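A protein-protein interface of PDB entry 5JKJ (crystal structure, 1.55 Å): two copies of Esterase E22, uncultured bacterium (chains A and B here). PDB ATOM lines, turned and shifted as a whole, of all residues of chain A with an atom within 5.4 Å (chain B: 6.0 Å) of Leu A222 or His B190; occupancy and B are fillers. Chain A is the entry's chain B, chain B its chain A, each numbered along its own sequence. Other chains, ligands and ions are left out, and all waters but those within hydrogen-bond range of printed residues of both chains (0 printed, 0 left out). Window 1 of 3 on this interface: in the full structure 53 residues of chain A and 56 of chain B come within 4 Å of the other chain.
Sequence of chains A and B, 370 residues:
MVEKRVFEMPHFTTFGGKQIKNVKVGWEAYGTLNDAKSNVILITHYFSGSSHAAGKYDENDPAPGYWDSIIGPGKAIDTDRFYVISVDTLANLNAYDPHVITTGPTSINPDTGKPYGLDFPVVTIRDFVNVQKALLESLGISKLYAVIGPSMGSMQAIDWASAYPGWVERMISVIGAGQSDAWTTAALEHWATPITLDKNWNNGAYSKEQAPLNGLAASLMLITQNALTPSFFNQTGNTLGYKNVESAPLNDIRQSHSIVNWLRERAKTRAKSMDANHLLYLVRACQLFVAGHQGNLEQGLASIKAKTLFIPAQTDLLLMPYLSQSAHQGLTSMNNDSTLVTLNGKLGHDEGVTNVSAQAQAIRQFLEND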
ATOM      1  N   HIS A 190      27.794 -21.761   6.813  1.00  0.00           N
ATOM      2  CA  HIS A 190      27.118 -22.694   5.915  1.00  0.00           C
ATOM      3  C   HIS A 190      28.054 -23.778   5.411  1.00  0.00           C
ATOM      4  O   HIS A 190      27.583 -24.827   4.948  1.00  0.00           O
ATOM      5  CB  HIS A 190      26.496 -21.938   4.739  1.00  0.00           C
ATOM      6  CG  HIS A 190      25.659 -20.781   5.169  1.00  0.00           C
ATOM      7  ND1 HIS A 190      24.553 -20.931   5.980  1.00  0.00           N
ATOM      8  CD2 HIS A 190      25.794 -19.455   4.951  1.00  0.00           C
ATOM      9  CE1 HIS A 190      24.031 -19.739   6.223  1.00  0.00           C
ATOM     10  NE2 HIS A 190      24.764 -18.828   5.606  1.00  0.00           N
ATOM     11  N   TRP A 191      29.365 -23.546   5.489  1.00  0.00           N
ATOM     12  CA  TRP A 191      30.329 -24.608   5.207  1.00  0.00           C
ATOM     13  C   TRP A 191      30.335 -25.662   6.297  1.00  0.00           C
ATOM     14  O   TRP A 191      30.712 -26.808   6.041  1.00  0.00           O
ATOM     15  CB  TRP A 191      31.741 -24.035   5.093  1.00  0.00           C
ATOM     16  CG  TRP A 191      31.957 -23.084   3.963  1.00  0.00           C
ATOM     17  CD1 TRP A 191      31.031 -22.617   3.077  1.00  0.00           C
ATOM     18  CD2 TRP A 191      33.200 -22.479   3.606  1.00  0.00           C
ATOM     19  NE1 TRP A 191      31.631 -21.776   2.171  1.00  0.00           N
ATOM     20  CE2 TRP A 191      32.961 -21.661   2.483  1.00  0.00           C
ATOM     21  CE3 TRP A 191      34.501 -22.569   4.115  1.00  0.00           C
ATOM     22  CZ2 TRP A 191      33.975 -20.941   1.855  1.00  0.00           C
ATOM     23  CZ3 TRP A 191      35.501 -21.856   3.495  1.00  0.00           C
ATOM     24  CH2 TRP A 191      35.237 -21.049   2.385  1.00  0.00           C
ATOM     25  N   ALA A 217      31.370 -33.818   1.572  1.00  0.00           N
ATOM     26  CA  ALA A 217      31.212 -33.508   0.152  1.00  0.00           C
ATOM     27  C   ALA A 217      30.262 -32.334  -0.048  1.00  0.00           C
ATOM     28  O   ALA A 217      30.522 -31.456  -0.878  1.00  0.00           O
ATOM     29  CB  ALA A 217      30.713 -34.739  -0.615  1.00  0.00           C
ATOM     30  N   ALA A 218      29.160 -32.297   0.708  1.00  0.00           N
ATOM     31  CA  ALA A 218      28.231 -31.168   0.610  1.00  0.00           C
ATOM     32  C   ALA A 218      28.911 -29.849   0.961  1.00  0.00           C
ATOM     33  O   ALA A 218      28.730 -28.842   0.268  1.00  0.00           O
ATOM     34  CB  ALA A 218      27.025 -31.403   1.519  1.00  0.00           C
ATOM     35  N   SER A 219      29.705 -29.837   2.032  1.00  0.00           N
ATOM     36  CA  SER A 219      30.490 -28.647   2.354  1.00  0.00           C
ATOM     37  C   SER A 219      31.384 -28.247   1.188  1.00  0.00           C
ATOM     38  O   SER A 219      31.448 -27.066   0.814  1.00  0.00           O
ATOM     39  CB  SER A 219      31.321 -28.907   3.607  1.00  0.00           C
ATOM     40  OG  SER A 219      30.468 -29.088   4.733  1.00  0.00           O
ATOM     41  N   LEU A 220      32.088 -29.222   0.596  1.00  0.00           N
ATOM     42  CA  LEU A 220      33.000 -28.881  -0.489  1.00  0.00           C
ATOM     43  C   LEU A 220      32.256 -28.440  -1.746  1.00  0.00           C
ATOM     44  O   LEU A 220      32.806 -27.661  -2.537  1.00  0.00           O
ATOM     45  CB  LEU A 220      33.924 -30.055  -0.811  1.00  0.00           C
ATOM     46  CG  LEU A 220      35.306 -30.040  -0.137  1.00  0.00           C
ATOM     47  CD1 LEU A 220      36.130 -28.818  -0.534  1.00  0.00           C
ATOM     48  CD2 LEU A 220      35.176 -30.115   1.370  1.00  0.00           C
ATOM     49  N   MET A 221      31.023 -28.912  -1.955  1.00  0.00           N
ATOM     50  CA  MET A 221      30.235 -28.401  -3.075  1.00  0.00           C
ATOM     51  C   MET A 221      29.980 -26.908  -2.919  1.00  0.00           C
ATOM     52  O   MET A 221      30.089 -26.148  -3.885  1.00  0.00           O
ATOM     53  CB  MET A 221      28.905 -29.140  -3.180  1.00  0.00           C
ATOM     54  CG  MET A 221      29.028 -30.573  -3.656  1.00  0.00           C
ATOM     55  SD  MET A 221      27.476 -31.499  -3.543  1.00  0.00           S
ATOM     56  CE  MET A 221      26.487 -30.761  -4.853  1.00  0.00           C
ATOM     57  N   LEU A 222      29.634 -26.477  -1.708  1.00  0.00           N
ATOM     58  CA  LEU A 222      29.359 -25.065  -1.467  1.00  0.00           C
ATOM     59  C   LEU A 222      30.642 -24.233  -1.528  1.00  0.00           C
ATOM     60  O   LEU A 222      30.671 -23.170  -2.170  1.00  0.00           O
ATOM     61  CB  LEU A 222      28.644 -24.930  -0.115  1.00  0.00           C
ATOM     62  CG  LEU A 222      28.140 -23.570   0.359  1.00  0.00           C
ATOM     63  CD1 LEU A 222      27.208 -22.926  -0.639  1.00  0.00           C
ATOM     64  CD2 LEU A 222      27.470 -23.715   1.727  1.00  0.00           C
ATOM     65  N   ILE A 223      31.725 -24.724  -0.911  1.00  0.00           N
ATOM     66  CA  ILE A 223      33.022 -24.047  -0.975  1.00  0.00           C
ATOM     67  C   ILE A 223      33.460 -23.867  -2.423  1.00  0.00           C
ATOM     68  O   ILE A 223      33.883 -22.778  -2.835  1.00  0.00           O
ATOM     69  CB  ILE A 223      34.071 -24.840  -0.174  1.00  0.00           C
ATOM     70  CG1 ILE A 223      33.770 -24.772   1.326  1.00  0.00           C
ATOM     71  CG2 ILE A 223      35.476 -24.337  -0.477  1.00  0.00           C
ATOM     72  CD1 ILE A 223      34.535 -25.786   2.157  1.00  0.00           C
ATOM     73  N   THR A 224      33.374 -24.941  -3.211  1.00  0.00           N
ATOM     74  CA  THR A 224      33.795 -24.892  -4.604  1.00  0.00           C
ATOM     75  C   THR A 224      33.023 -23.831  -5.373  1.00  0.00           C
ATOM     76  O   THR A 224      33.617 -23.037  -6.111  1.00  0.00           O
ATOM     77  CB  THR A 224      33.619 -26.274  -5.238  1.00  0.00           C
ATOM     78  OG1 THR A 224      34.506 -27.199  -4.591  1.00  0.00           O
ATOM     79  CG2 THR A 224      33.922 -26.241  -6.743  1.00  0.00           C
ATOM     80  N   GLN A 225      31.699 -23.781  -5.194  1.00  0.00           N
ATOM     81  CA  GLN A 225      30.925 -22.804  -5.950  1.00  0.00           C
ATOM     82  C   GLN A 225      31.151 -21.388  -5.429  1.00  0.00           C
ATOM     83  O   GLN A 225      31.294 -20.454  -6.227  1.00  0.00           O
ATOM     84  CB  GLN A 225      29.435 -23.152  -5.931  1.00  0.00           C
ATOM     85  CG  GLN A 225      28.610 -22.094  -6.666  1.00  0.00           C
ATOM     86  CD  GLN A 225      27.248 -22.571  -7.101  1.00  0.00           C
ATOM     87  OE1 GLN A 225      26.739 -23.597  -6.631  1.00  0.00           O
ATOM     88  NE2 GLN A 225      26.640 -21.828  -8.027  1.00  0.00           N
ATOM     89  N   ASN A 226      31.188 -21.210  -4.096  1.00  0.00           N
ATOM     90  CA  ASN A 226      31.405 -19.886  -3.510  1.00  0.00           C
ATOM     91  C   ASN A 226      32.679 -19.243  -4.038  1.00  0.00           C
ATOM     92  O   ASN A 226      32.762 -18.012  -4.152  1.00  0.00           O
ATOM     93  CB  ASN A 226      31.530 -19.967  -1.978  1.00  0.00           C
ATOM     94  CG  ASN A 226      30.205 -20.203  -1.240  1.00  0.00           C
ATOM     95  OD1 ASN A 226      30.224 -20.474  -0.029  1.00  0.00           O
ATOM     96  ND2 ASN A 226      29.074 -20.091  -1.929  1.00  0.00           N
ATOM     97  N   ALA A 227      33.687 -20.055  -4.342  1.00  0.00           N
ATOM     98  CA  ALA A 227      34.991 -19.547  -4.742  1.00  0.00           C
ATOM     99  C   ALA A 227      35.102 -19.324  -6.238  1.00  0.00           C
ATOM    100  O   ALA A 227      36.178 -18.953  -6.708  1.00  0.00           O
ATOM    101  CB  ALA A 227      36.092 -20.515  -4.284  1.00  0.00           C
ATOM    102  N   LEU A 263      29.329 -30.999 -10.050  1.00  0.00           N
ATOM    103  CA  LEU A 263      29.817 -30.352  -8.833  1.00  0.00           C
ATOM    104  C   LEU A 263      29.965 -31.355  -7.698  1.00  0.00           C
ATOM    105  O   LEU A 263      30.936 -31.296  -6.930  1.00  0.00           O
ATOM    106  CB  LEU A 263      28.870 -29.220  -8.425  1.00  0.00           C
ATOM    107  CG  LEU A 263      29.271 -28.407  -7.181  1.00  0.00           C
ATOM    108  CD1 LEU A 263      30.658 -27.810  -7.362  1.00  0.00           C
ATOM    109  CD2 LEU A 263      28.248 -27.302  -6.875  1.00  0.00           C
ATOM    110  N   THR B 185      21.185 -23.129 -10.921  1.00  0.00           N
ATOM    111  CA  THR B 185      20.767 -24.479 -10.568  1.00  0.00           C
ATOM    112  C   THR B 185      21.700 -25.099  -9.533  1.00  0.00           C
ATOM    113  O   THR B 185      21.239 -25.758  -8.589  1.00  0.00           O
ATOM    114  CB  THR B 185      20.662 -25.324 -11.835  1.00  0.00           C
ATOM    115  OG1 THR B 185      19.444 -24.956 -12.490  1.00  0.00           O
ATOM    116  CG2 THR B 185      20.632 -26.813 -11.517  1.00  0.00           C
ATOM    117  N   ALA B 186      23.006 -24.869  -9.664  1.00  0.00           N
ATOM    118  CA  ALA B 186      23.935 -25.369  -8.657  1.00  0.00           C
ATOM    119  C   ALA B 186      23.748 -24.635  -7.334  1.00  0.00           C
ATOM    120  O   ALA B 186      23.776 -25.262  -6.272  1.00  0.00           O
ATOM    121  CB  ALA B 186      25.372 -25.238  -9.156  1.00  0.00           C
ATOM    122  N   ALA B 187      23.519 -23.315  -7.388  1.00  0.00           N
ATOM    123  CA  ALA B 187      23.334 -22.531  -6.166  1.00  0.00           C
ATOM    124  C   ALA B 187      22.108 -22.995  -5.384  1.00  0.00           C
ATOM    125  O   ALA B 187      22.149 -23.106  -4.148  1.00  0.00           O
ATOM    126  CB  ALA B 187      23.213 -21.048  -6.513  1.00  0.00           C
ATOM    127  N   LEU B 188      21.008 -23.275  -6.091  1.00  0.00           N
ATOM    128  CA  LEU B 188      19.782 -23.729  -5.442  1.00  0.00           C
ATOM    129  C   LEU B 188      19.950 -25.115  -4.843  1.00  0.00           C
ATOM    130  O   LEU B 188      19.282 -25.450  -3.860  1.00  0.00           O
ATOM    131  CB  LEU B 188      18.628 -23.727  -6.449  1.00  0.00           C
ATOM    132  CG  LEU B 188      18.135 -22.351  -6.881  1.00  0.00           C
ATOM    133  CD1 LEU B 188      17.293 -22.451  -8.148  1.00  0.00           C
ATOM    134  CD2 LEU B 188      17.318 -21.740  -5.761  1.00  0.00           C
ATOM    135  N   GLU B 189      20.813 -25.946  -5.431  1.00  0.00           N
ATOM    136  CA  GLU B 189      21.006 -27.283  -4.889  1.00  0.00           C
ATOM    137  C   GLU B 189      21.477 -27.234  -3.445  1.00  0.00           C
ATOM    138  O   GLU B 189      21.107 -28.100  -2.647  1.00  0.00           O
ATOM    139  CB  GLU B 189      22.006 -28.064  -5.738  1.00  0.00           C
ATOM    140  CG  GLU B 189      22.152 -29.531  -5.330  1.00  0.00           C
ATOM    141  CD  GLU B 189      20.950 -30.392  -5.693  1.00  0.00           C
ATOM    142  OE1 GLU B 189      20.066 -29.940  -6.460  1.00  0.00           O
ATOM    143  OE2 GLU B 189      20.899 -31.549  -5.219  1.00  0.00           O
ATOM    144  N   HIS B 190      22.276 -26.227  -3.082  1.00  0.00           N
ATOM    145  CA  HIS B 190      22.752 -26.156  -1.703  1.00  0.00           C
ATOM    146  C   HIS B 190      21.629 -25.876  -0.719  1.00  0.00           C
ATOM    147  O   HIS B 190      21.807 -26.128   0.472  1.00  0.00           O
ATOM    148  CB  HIS B 190      23.844 -25.093  -1.561  1.00  0.00           C
ATOM    149  CG  HIS B 190      24.892 -25.183  -2.617  1.00  0.00           C
ATOM    150  ND1 HIS B 190      25.541 -26.361  -2.917  1.00  0.00           N
ATOM    151  CD2 HIS B 190      25.367 -24.256  -3.481  1.00  0.00           C
ATOM    152  CE1 HIS B 190      26.391 -26.147  -3.906  1.00  0.00           C
ATOM    153  NE2 HIS B 190      26.297 -24.881  -4.273  1.00  0.00           N
ATOM    154  N   TRP B 191      20.485 -25.362  -1.184  1.00  0.00           N
ATOM    155  CA  TRP B 191      19.320 -25.223  -0.307  1.00  0.00           C
ATOM    156  C   TRP B 191      18.724 -26.578   0.036  1.00  0.00           C
ATOM    157  O   TRP B 191      18.087 -26.732   1.085  1.00  0.00           O
ATOM    158  CB  TRP B 191      18.228 -24.374  -0.967  1.00  0.00           C
ATOM    159  CG  TRP B 191      18.595 -22.957  -1.268  1.00  0.00           C
ATOM    160  CD1 TRP B 191      19.800 -22.347  -1.046  1.00  0.00           C
ATOM    161  CD2 TRP B 191      17.731 -21.953  -1.816  1.00  0.00           C
ATOM    162  NE1 TRP B 191      19.738 -21.033  -1.434  1.00  0.00           N
ATOM    163  CE2 TRP B 191      18.478 -20.765  -1.907  1.00  0.00           C
ATOM    164  CE3 TRP B 191      16.392 -21.941  -2.217  1.00  0.00           C
ATOM    165  CZ2 TRP B 191      17.936 -19.578  -2.402  1.00  0.00           C
ATOM    166  CZ3 TRP B 191      15.856 -20.762  -2.700  1.00  0.00           C
ATOM    167  CH2 TRP B 191      16.621 -19.603  -2.799  1.00  0.00           C
ATOM    168  N   ALA B 192      18.893 -27.557  -0.852  1.00  0.00           N
ATOM    169  CA  ALA B 192      18.290 -28.874  -0.668  1.00  0.00           C
ATOM    170  C   ALA B 192      19.149 -29.783   0.194  1.00  0.00           C
ATOM    171  O   ALA B 192      18.623 -30.532   1.028  1.00  0.00           O
ATOM    172  CB  ALA B 192      18.058 -29.527  -2.036  1.00  0.00           C
ATOM    173  N   THR B 193      20.469 -29.737   0.004  1.00  0.00           N
ATOM    174  CA  THR B 193      21.334 -30.744   0.611  1.00  0.00           C
ATOM    175  C   THR B 193      21.221 -30.837   2.132  1.00  0.00           C
ATOM    176  O   THR B 193      21.220 -31.970   2.647  1.00  0.00           O
ATOM    177  CB  THR B 193      22.780 -30.500   0.174  1.00  0.00           C
ATOM    178  OG1 THR B 193      22.814 -30.379  -1.260  1.00  0.00           O
ATOM    179  CG2 THR B 193      23.637 -31.666   0.576  1.00  0.00           C
ATOM    180  N   PRO B 194      21.093 -29.747   2.898  1.00  0.00           N
ATOM    181  CA  PRO B 194      21.006 -29.924   4.363  1.00  0.00           C
ATOM    182  C   PRO B 194      19.825 -30.777   4.787  1.00  0.00           C
ATOM    183  O   PRO B 194      19.937 -31.566   5.734  1.00  0.00           O
ATOM    184  CB  PRO B 194      20.904 -28.482   4.882  1.00  0.00           C
ATOM    185  CG  PRO B 194      21.589 -27.650   3.800  1.00  0.00           C
ATOM    186  CD  PRO B 194      21.160 -28.320   2.526  1.00  0.00           C
ATOM    187  N   SER B 219      18.924 -25.113   5.874  1.00  0.00           N
ATOM    188  CA  SER B 219      18.509 -24.618   4.570  1.00  0.00           C
ATOM    189  C   SER B 219      18.032 -23.179   4.661  1.00  0.00           C
ATOM    190  O   SER B 219      18.405 -22.335   3.834  1.00  0.00           O
ATOM    191  CB  SER B 219      17.395 -25.505   4.012  1.00  0.00           C
ATOM    192  OG  SER B 219      17.876 -26.809   3.738  1.00  0.00           O
ATOM    193  N   LEU B 222      20.763 -20.569   4.984  1.00  0.00           N
ATOM    194  CA  LEU B 222      21.441 -20.262   3.730  1.00  0.00           C
ATOM    195  C   LEU B 222      20.551 -19.430   2.810  1.00  0.00           C
ATOM    196  O   LEU B 222      21.010 -18.446   2.220  1.00  0.00           O
ATOM    197  CB  LEU B 222      21.864 -21.567   3.058  1.00  0.00           C
ATOM    198  CG  LEU B 222      22.603 -21.477   1.731  1.00  0.00           C
ATOM    199  CD1 LEU B 222      23.850 -20.615   1.875  1.00  0.00           C
ATOM    200  CD2 LEU B 222      22.960 -22.880   1.266  1.00  0.00           C
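The backbone carbonyl oxygen of Ala B186 lies close to the side-chain amide oxygen of Gln A225.
N of Ala B187 lies within hydrogen-bond range of OE1 of Gln A225, at 3.3 Å.
OE1 of Gln A225 is in hydrogen-bond range of NE2 of His B190, 2.7 Å away.
O of Ala B186 sits at hydrogen-bond distance from NE2 of His B190, at 3.2 Å.
O of Glu B189 lies within hydrogen-bond range of OG1 of Thr B193 (3.2 Å).
O of Leu A222 lies close to OD1 of Asn A226, at 3.5 Å.
Among the printed residues, merely in contact across the chains: His A190 with Leu B222 (3.6 Å), Ala A218 with Thr B193 (3.5 Å), Met A221 with His B190 (3.7 Å), Leu A222 with His B190 (3.6 Å) and Leu A263 with His B190 (3.7 Å).
Of the printed residues of chain B, Ala A218 touches Thr B193.
Leu A220 touches none of the printed residues of chain B.
Of the printed residues of chain B, Met A221 touches His B190 (3.7 Å).
Of chain B, only His B190 (3.6 Å) comes within 4 Å of Leu A222.
Thr A224 touches none of the printed residues of chain B.
Printed residues of chain A within 4 Å of Ala B187: Gln A225.
His B190 touches just these residues of chain A: Met A221, Leu A222, Gln A225 and Leu A263.
The nearest residue of chain A that does not touch His B190 is Ala A218 (5.1 Å).
Of the 12 printed residues of chain B, 5 touch a printed residue of chain A.
Hydrophobic or aromatic side chains of chain A that line the printed part of chain B: His A190, Ala A218, Met A221, Leu A222 and Leu A263.
Among the printed residues, 8 pairs touch across the chains.
His A190 touches Leu B222, and with the chains exchanged Leu A222 touches His B190.
4 positions are printed for both chains.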
